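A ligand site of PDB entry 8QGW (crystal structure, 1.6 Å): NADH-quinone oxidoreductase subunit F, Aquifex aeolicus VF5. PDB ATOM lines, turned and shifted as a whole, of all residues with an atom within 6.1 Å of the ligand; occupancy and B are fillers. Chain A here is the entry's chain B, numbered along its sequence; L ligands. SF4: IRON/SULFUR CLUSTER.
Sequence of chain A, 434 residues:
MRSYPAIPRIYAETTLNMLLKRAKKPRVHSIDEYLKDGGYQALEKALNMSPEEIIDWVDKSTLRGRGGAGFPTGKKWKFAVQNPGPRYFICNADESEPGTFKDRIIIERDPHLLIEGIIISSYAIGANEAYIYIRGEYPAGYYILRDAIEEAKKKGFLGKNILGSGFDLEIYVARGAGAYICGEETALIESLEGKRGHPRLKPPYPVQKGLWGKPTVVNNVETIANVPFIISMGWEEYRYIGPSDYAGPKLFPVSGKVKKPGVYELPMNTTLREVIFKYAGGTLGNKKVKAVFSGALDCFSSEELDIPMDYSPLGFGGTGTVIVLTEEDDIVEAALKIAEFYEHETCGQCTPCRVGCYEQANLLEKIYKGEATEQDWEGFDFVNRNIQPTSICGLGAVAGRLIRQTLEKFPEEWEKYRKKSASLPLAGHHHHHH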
ATOM      1  N   ILE A 181     -32.711  30.785  28.753  1.00  0.00           N
ATOM      2  CA  ILE A 181     -33.373  30.585  27.466  1.00  0.00           C
ATOM      3  C   ILE A 181     -34.889  30.642  27.652  1.00  0.00           C
ATOM      4  O   ILE A 181     -35.610  30.885  26.707  1.00  0.00           O
ATOM      5  CB  ILE A 181     -32.927  29.288  26.764  1.00  0.00           C
ATOM      6  CG1 ILE A 181     -33.371  29.239  25.296  1.00  0.00           C
ATOM      7  CG2 ILE A 181     -33.398  28.042  27.502  1.00  0.00           C
ATOM      8  CD1 ILE A 181     -32.884  30.412  24.482  1.00  0.00           C
ATOM      9  N   HIS A 198     -37.150  24.684  25.333  1.00  0.00           N
ATOM     10  CA  HIS A 198     -36.569  24.587  24.019  1.00  0.00           C
ATOM     11  C   HIS A 198     -37.334  25.511  23.067  1.00  0.00           C
ATOM     12  O   HIS A 198     -38.513  25.262  22.780  1.00  0.00           O
ATOM     13  CB  HIS A 198     -36.646  23.152  23.493  1.00  0.00           C
ATOM     14  CG  HIS A 198     -35.666  22.240  24.153  1.00  0.00           C
ATOM     15  ND1 HIS A 198     -35.758  20.869  24.017  1.00  0.00           N
ATOM     16  CD2 HIS A 198     -34.620  22.468  24.945  1.00  0.00           C
ATOM     17  CE1 HIS A 198     -34.770  20.315  24.721  1.00  0.00           C
ATOM     18  NE2 HIS A 198     -34.081  21.251  25.303  1.00  0.00           N
ATOM     19  N   PRO A 199     -36.691  26.562  22.530  1.00  0.00           N
ATOM     20  CA  PRO A 199     -37.327  27.402  21.514  1.00  0.00           C
ATOM     21  C   PRO A 199     -37.885  26.604  20.340  1.00  0.00           C
ATOM     22  O   PRO A 199     -37.350  25.551  19.980  1.00  0.00           O
ATOM     23  CB  PRO A 199     -36.195  28.320  21.014  1.00  0.00           C
ATOM     24  CG  PRO A 199     -35.293  28.431  22.243  1.00  0.00           C
ATOM     25  CD  PRO A 199     -35.328  27.038  22.863  1.00  0.00           C
ATOM     26  N   GLU A 345     -25.863  28.904  28.885  1.00  0.00           N
ATOM     27  CA  GLU A 345     -27.277  29.116  28.601  1.00  0.00           C
ATOM     28  C   GLU A 345     -27.760  28.533  27.270  1.00  0.00           C
ATOM     29  O   GLU A 345     -28.968  28.397  27.088  1.00  0.00           O
ATOM     30  CB  GLU A 345     -27.610  30.594  28.753  1.00  0.00           C
ATOM     31  CG  GLU A 345     -27.339  31.098  30.169  1.00  0.00           C
ATOM     32  CD  GLU A 345     -28.051  30.400  31.316  1.00  0.00           C
ATOM     33  OE1 GLU A 345     -29.097  29.736  31.085  1.00  0.00           O
ATOM     34  OE2 GLU A 345     -27.522  30.470  32.465  1.00  0.00           O
ATOM     35  N   THR A 346     -26.854  28.148  26.355  1.00  0.00           N
ATOM     36  CA  THR A 346     -27.346  27.481  25.149  1.00  0.00           C
ATOM     37  C   THR A 346     -28.194  26.271  25.530  1.00  0.00           C
ATOM     38  O   THR A 346     -27.791  25.480  26.380  1.00  0.00           O
ATOM     39  CB  THR A 346     -26.240  27.042  24.189  1.00  0.00           C
ATOM     40  OG1 THR A 346     -26.828  26.210  23.188  1.00  0.00           O
ATOM     41  CG2 THR A 346     -25.113  26.283  24.854  1.00  0.00           C
ATOM     42  N   CYS A 347     -29.322  26.073  24.836  1.00  0.00           N
ATOM     43  CA  CYS A 347     -30.177  24.933  25.133  1.00  0.00           C
ATOM     44  C   CYS A 347     -29.735  23.644  24.437  1.00  0.00           C
ATOM     45  O   CYS A 347     -30.191  22.550  24.791  1.00  0.00           O
ATOM     46  CB  CYS A 347     -31.658  25.205  24.845  1.00  0.00           C
ATOM     47  SG  CYS A 347     -32.141  25.064  23.116  1.00  0.00           S
ATOM     48  N   GLY A 348     -28.852  23.757  23.422  1.00  0.00           N
ATOM     49  CA  GLY A 348     -28.212  22.608  22.808  1.00  0.00           C
ATOM     50  C   GLY A 348     -28.958  21.974  21.633  1.00  0.00           C
ATOM     51  O   GLY A 348     -28.470  21.010  21.056  1.00  0.00           O
ATOM     52  N   GLN A 349     -30.130  22.508  21.239  1.00  0.00           N
ATOM     53  CA  GLN A 349     -30.902  21.936  20.145  1.00  0.00           C
ATOM     54  C   GLN A 349     -30.170  22.056  18.809  1.00  0.00           C
ATOM     55  O   GLN A 349     -30.326  21.198  17.934  1.00  0.00           O
ATOM     56  CB  GLN A 349     -32.262  22.627  19.929  1.00  0.00           C
ATOM     57  CG  GLN A 349     -33.341  22.320  20.935  1.00  0.00           C
ATOM     58  CD  GLN A 349     -34.607  22.976  20.410  1.00  0.00           C
ATOM     59  OE1 GLN A 349     -35.382  22.350  19.671  1.00  0.00           O
ATOM     60  NE2 GLN A 349     -34.765  24.268  20.694  1.00  0.00           N
ATOM     61  N   CYS A 350     -29.428  23.151  18.631  1.00  0.00           N
ATOM     62  CA  CYS A 350     -28.794  23.465  17.362  1.00  0.00           C
ATOM     63  C   CYS A 350     -27.290  23.195  17.516  1.00  0.00           C
ATOM     64  O   CYS A 350     -26.682  23.598  18.519  1.00  0.00           O
ATOM     65  CB  CYS A 350     -29.039  24.915  16.963  1.00  0.00           C
ATOM     66  SG  CYS A 350     -30.759  25.491  17.156  1.00  0.00           S
ATOM     67  N   THR A 351     -26.707  22.534  16.525  1.00  0.00           N
ATOM     68  CA  THR A 351     -25.332  22.052  16.656  1.00  0.00           C
ATOM     69  C   THR A 351     -24.337  23.214  16.726  1.00  0.00           C
ATOM     70  O   THR A 351     -23.493  23.199  17.609  1.00  0.00           O
ATOM     71  CB  THR A 351     -25.026  20.960  15.613  1.00  0.00           C
ATOM     72  OG1 THR A 351     -25.735  19.797  16.024  1.00  0.00           O
ATOM     73  CG2 THR A 351     -23.547  20.647  15.504  1.00  0.00           C
ATOM     74  N   CYS A 353     -24.673  26.304  17.642  1.00  0.00           N
ATOM     75  CA  CYS A 353     -24.859  26.983  18.915  1.00  0.00           C
ATOM     76  C   CYS A 353     -24.330  26.128  20.070  1.00  0.00           C
ATOM     77  O   CYS A 353     -23.597  26.619  20.923  1.00  0.00           O
ATOM     78  CB  CYS A 353     -26.326  27.309  19.131  1.00  0.00           C
ATOM     79  SG  CYS A 353     -26.685  28.232  20.644  1.00  0.00           S
ATOM     80  N   ARG A 354     -24.717  24.870  20.121  1.00  0.00           N
ATOM     81  CA  ARG A 354     -24.312  23.979  21.206  1.00  0.00           C
ATOM     82  C   ARG A 354     -22.783  23.915  21.322  1.00  0.00           C
ATOM     83  O   ARG A 354     -22.189  24.121  22.394  1.00  0.00           O
ATOM     84  CB  ARG A 354     -24.863  22.575  20.963  1.00  0.00           C
ATOM     85  CG  ARG A 354     -24.463  21.529  22.011  1.00  0.00           C
ATOM     86  CD  ARG A 354     -25.145  20.195  21.735  1.00  0.00           C
ATOM     87  NE  ARG A 354     -24.681  19.563  20.512  1.00  0.00           N
ATOM     88  CZ  ARG A 354     -25.317  19.426  19.367  1.00  0.00           C
ATOM     89  NH1 ARG A 354     -26.566  19.887  19.218  1.00  0.00           N
ATOM     90  NH2 ARG A 354     -24.675  18.786  18.377  1.00  0.00           N
ATOM     91  N   CYS A 357     -20.981  27.795  21.493  1.00  0.00           N
ATOM     92  CA  CYS A 357     -20.974  28.478  22.787  1.00  0.00           C
ATOM     93  C   CYS A 357     -19.987  27.808  23.765  1.00  0.00           C
ATOM     94  O   CYS A 357     -19.279  28.487  24.507  1.00  0.00           O
ATOM     95  CB  CYS A 357     -22.357  28.526  23.416  1.00  0.00           C
ATOM     96  SG  CYS A 357     -23.532  29.577  22.518  1.00  0.00           S
ATOM     97  N   THR A 390     -27.719  27.832  11.252  1.00  0.00           N
ATOM     98  CA  THR A 390     -28.803  26.889  11.524  1.00  0.00           C
ATOM     99  C   THR A 390     -29.532  27.186  12.838  1.00  0.00           C
ATOM    100  O   THR A 390     -30.505  26.483  13.154  1.00  0.00           O
ATOM    101  CB  THR A 390     -28.338  25.422  11.487  1.00  0.00           C
ATOM    102  OG1 THR A 390     -27.786  25.065  12.750  1.00  0.00           O
ATOM    103  CG2 THR A 390     -27.339  25.144  10.387  1.00  0.00           C
ATOM    104  N   SER A 391     -29.117  28.217  13.593  1.00  0.00           N
ATOM    105  CA  SER A 391     -29.758  28.555  14.847  1.00  0.00           C
ATOM    106  C   SER A 391     -31.254  28.823  14.667  1.00  0.00           C
ATOM    107  O   SER A 391     -31.673  29.500  13.713  1.00  0.00           O
ATOM    108  CB  SER A 391     -29.047  29.720  15.493  1.00  0.00           C
ATOM    109  OG  SER A 391     -29.133  30.882  14.676  1.00  0.00           O
ATOM    110  N   ILE A 392     -32.080  28.322  15.600  1.00  0.00           N
ATOM    111  CA  ILE A 392     -33.511  28.622  15.502  1.00  0.00           C
ATOM    112  C   ILE A 392     -33.946  29.750  16.427  1.00  0.00           C
ATOM    113  O   ILE A 392     -35.138  30.104  16.396  1.00  0.00           O
ATOM    114  CB  ILE A 392     -34.365  27.352  15.658  1.00  0.00           C
ATOM    115  CG1 ILE A 392     -34.187  26.623  16.975  1.00  0.00           C
ATOM    116  CG2 ILE A 392     -34.082  26.430  14.479  1.00  0.00           C
ATOM    117  CD1 ILE A 392     -34.937  25.292  16.998  1.00  0.00           C
ATOM    118  N   CYS A 393     -33.069  30.276  17.313  1.00  0.00           N
ATOM    119  CA  CYS A 393     -33.479  31.395  18.157  1.00  0.00           C
ATOM    120  C   CYS A 393     -32.353  32.416  18.245  1.00  0.00           C
ATOM    121  O   CYS A 393     -31.244  32.228  17.734  1.00  0.00           O
ATOM    122  CB  CYS A 393     -33.943  30.962  19.557  1.00  0.00           C
ATOM    123  SG  CYS A 393     -32.654  30.861  20.831  1.00  0.00           S
ATOM    124  N   GLY A 394     -32.680  33.548  18.875  1.00  0.00           N
ATOM    125  CA  GLY A 394     -31.770  34.690  18.922  1.00  0.00           C
ATOM    126  C   GLY A 394     -30.469  34.437  19.659  1.00  0.00           C
ATOM    127  O   GLY A 394     -29.511  35.189  19.451  1.00  0.00           O
ATOM    128  N   LEU A 395     -30.434  33.447  20.574  1.00  0.00           N
ATOM    129  CA  LEU A 395     -29.243  33.249  21.390  1.00  0.00           C
ATOM    130  C   LEU A 395     -28.073  32.878  20.464  1.00  0.00           C
ATOM    131  O   LEU A 395     -27.009  33.508  20.511  1.00  0.00           O
ATOM    132  CB  LEU A 395     -29.485  32.200  22.481  1.00  0.00           C
ATOM    133  CG  LEU A 395     -28.350  32.036  23.506  1.00  0.00           C
ATOM    134  CD1 LEU A 395     -28.892  31.538  24.838  1.00  0.00           C
ATOM    135  CD2 LEU A 395     -27.318  31.027  23.003  1.00  0.00           C
ATOM    136  N   GLY A 396     -28.264  31.886  19.594  1.00  0.00           N
ATOM    137  CA  GLY A 396     -27.197  31.494  18.670  1.00  0.00           C
ATOM    138  C   GLY A 396     -26.794  32.607  17.718  1.00  0.00           C
ATOM    139  O   GLY A 396     -25.633  32.745  17.350  1.00  0.00           O
ATOM    140  N   ALA A 397     -27.751  33.475  17.382  1.00  0.00           N
ATOM    141  CA  ALA A 397     -27.499  34.588  16.496  1.00  0.00           C
ATOM    142  C   ALA A 397     -26.594  35.636  17.138  1.00  0.00           C
ATOM    143  O   ALA A 397     -25.898  36.333  16.396  1.00  0.00           O
ATOM    144  CB  ALA A 397     -28.786  35.197  15.999  1.00  0.00           C
HETATM  145 FE1  SF4 L   1     -31.099  26.515  21.734  1.00  0.00          FE
HETATM  146 FE2  SF4 L   1     -28.959  27.965  20.709  1.00  0.00          FE
HETATM  147 FE3  SF4 L   1     -31.497  28.947  20.503  1.00  0.00          FE
HETATM  148 FE4  SF4 L   1     -30.701  26.747  19.064  1.00  0.00          FE
HETATM  149  S1  SF4 L   1     -29.937  28.941  18.868  1.00  0.00           S
HETATM  150  S2  SF4 L   1     -32.690  27.002  20.117  1.00  0.00           S
HETATM  151  S3  SF4 L   1     -29.312  25.706  20.576  1.00  0.00           S
HETATM  152  S4  SF4 L   1     -30.295  28.554  22.444  1.00  0.00           S
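Ile 181 touches the ligand. Pro 199 touches the ligand. Ser 391 touches the ligand. Ile 392 touches the ligand (CG1 to S2, 3.5 Å). Leu 395 touches the ligand (CB to S4, 3.7 Å). Of the 21 residues printed, 13 come within 4 Å of the ligand.
A sulfur (S4) of the ligand sits close to the backbone NH (N) of Cys 347 (3.6 Å). FE1 of the ligand is bound by SG of Cys 347. N of Cys 393 lies close to S1 of the ligand. The side-chain sulfur of Cys 393 is bound to an iron atom (FE3) of the ligand. S3 of the ligand lies close to N of Cys 350 (3.2 Å). An iron atom (FE4) of the ligand is bound by the side-chain sulfur of Cys 350 (2.3 Å). SG of Cys 353 is bound to FE2 of the ligand, at 2.3 Å. N of Gln 349 sits close to S3 of the ligand (3.4 Å). A sulfur (S2) of the ligand sits close to the side-chain amide nitrogen (NE2) of Gln 349, at 3.5 Å. S1 of the ligand lies close to N of Gly 396. S3 of the ligand lies close to N of Gly 348 (3.5 Å). OG1 of Thr 346 lies close to S3 of the ligand.
SG of Cys 347 lies close to NE2 of Gln 349 (3.7 Å). The backbone NH of Leu 395 lies close to the side-chain sulfur of Cys 393, at 3.4 Å. The backbone NH (N) of Ile 392 lies close to the side-chain sulfur (SG) of Cys 350 (3.5 Å). The side-chain sulfur (SG) of Cys 353 sits close to the side-chain hydroxyl (OG1) of Thr 346, 3.3 Å away. The side-chain sulfur (SG) of Cys 357 lies within hydrogen-bond range of the backbone carbonyl oxygen (O) of Cys 353 (3.4 Å). The side-chain amide nitrogen (NE2) of Gln 349 is in hydrogen-bond range of the backbone carbonyl oxygen (O) of Pro 199 (3.0 Å). N of Gly 348 lies within hydrogen-bond range of OG1 of Thr 346, 3.2 Å away. O of Gly 348 sits at hydrogen-bond distance from NH1 of Arg 354, 2.9 Å away.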
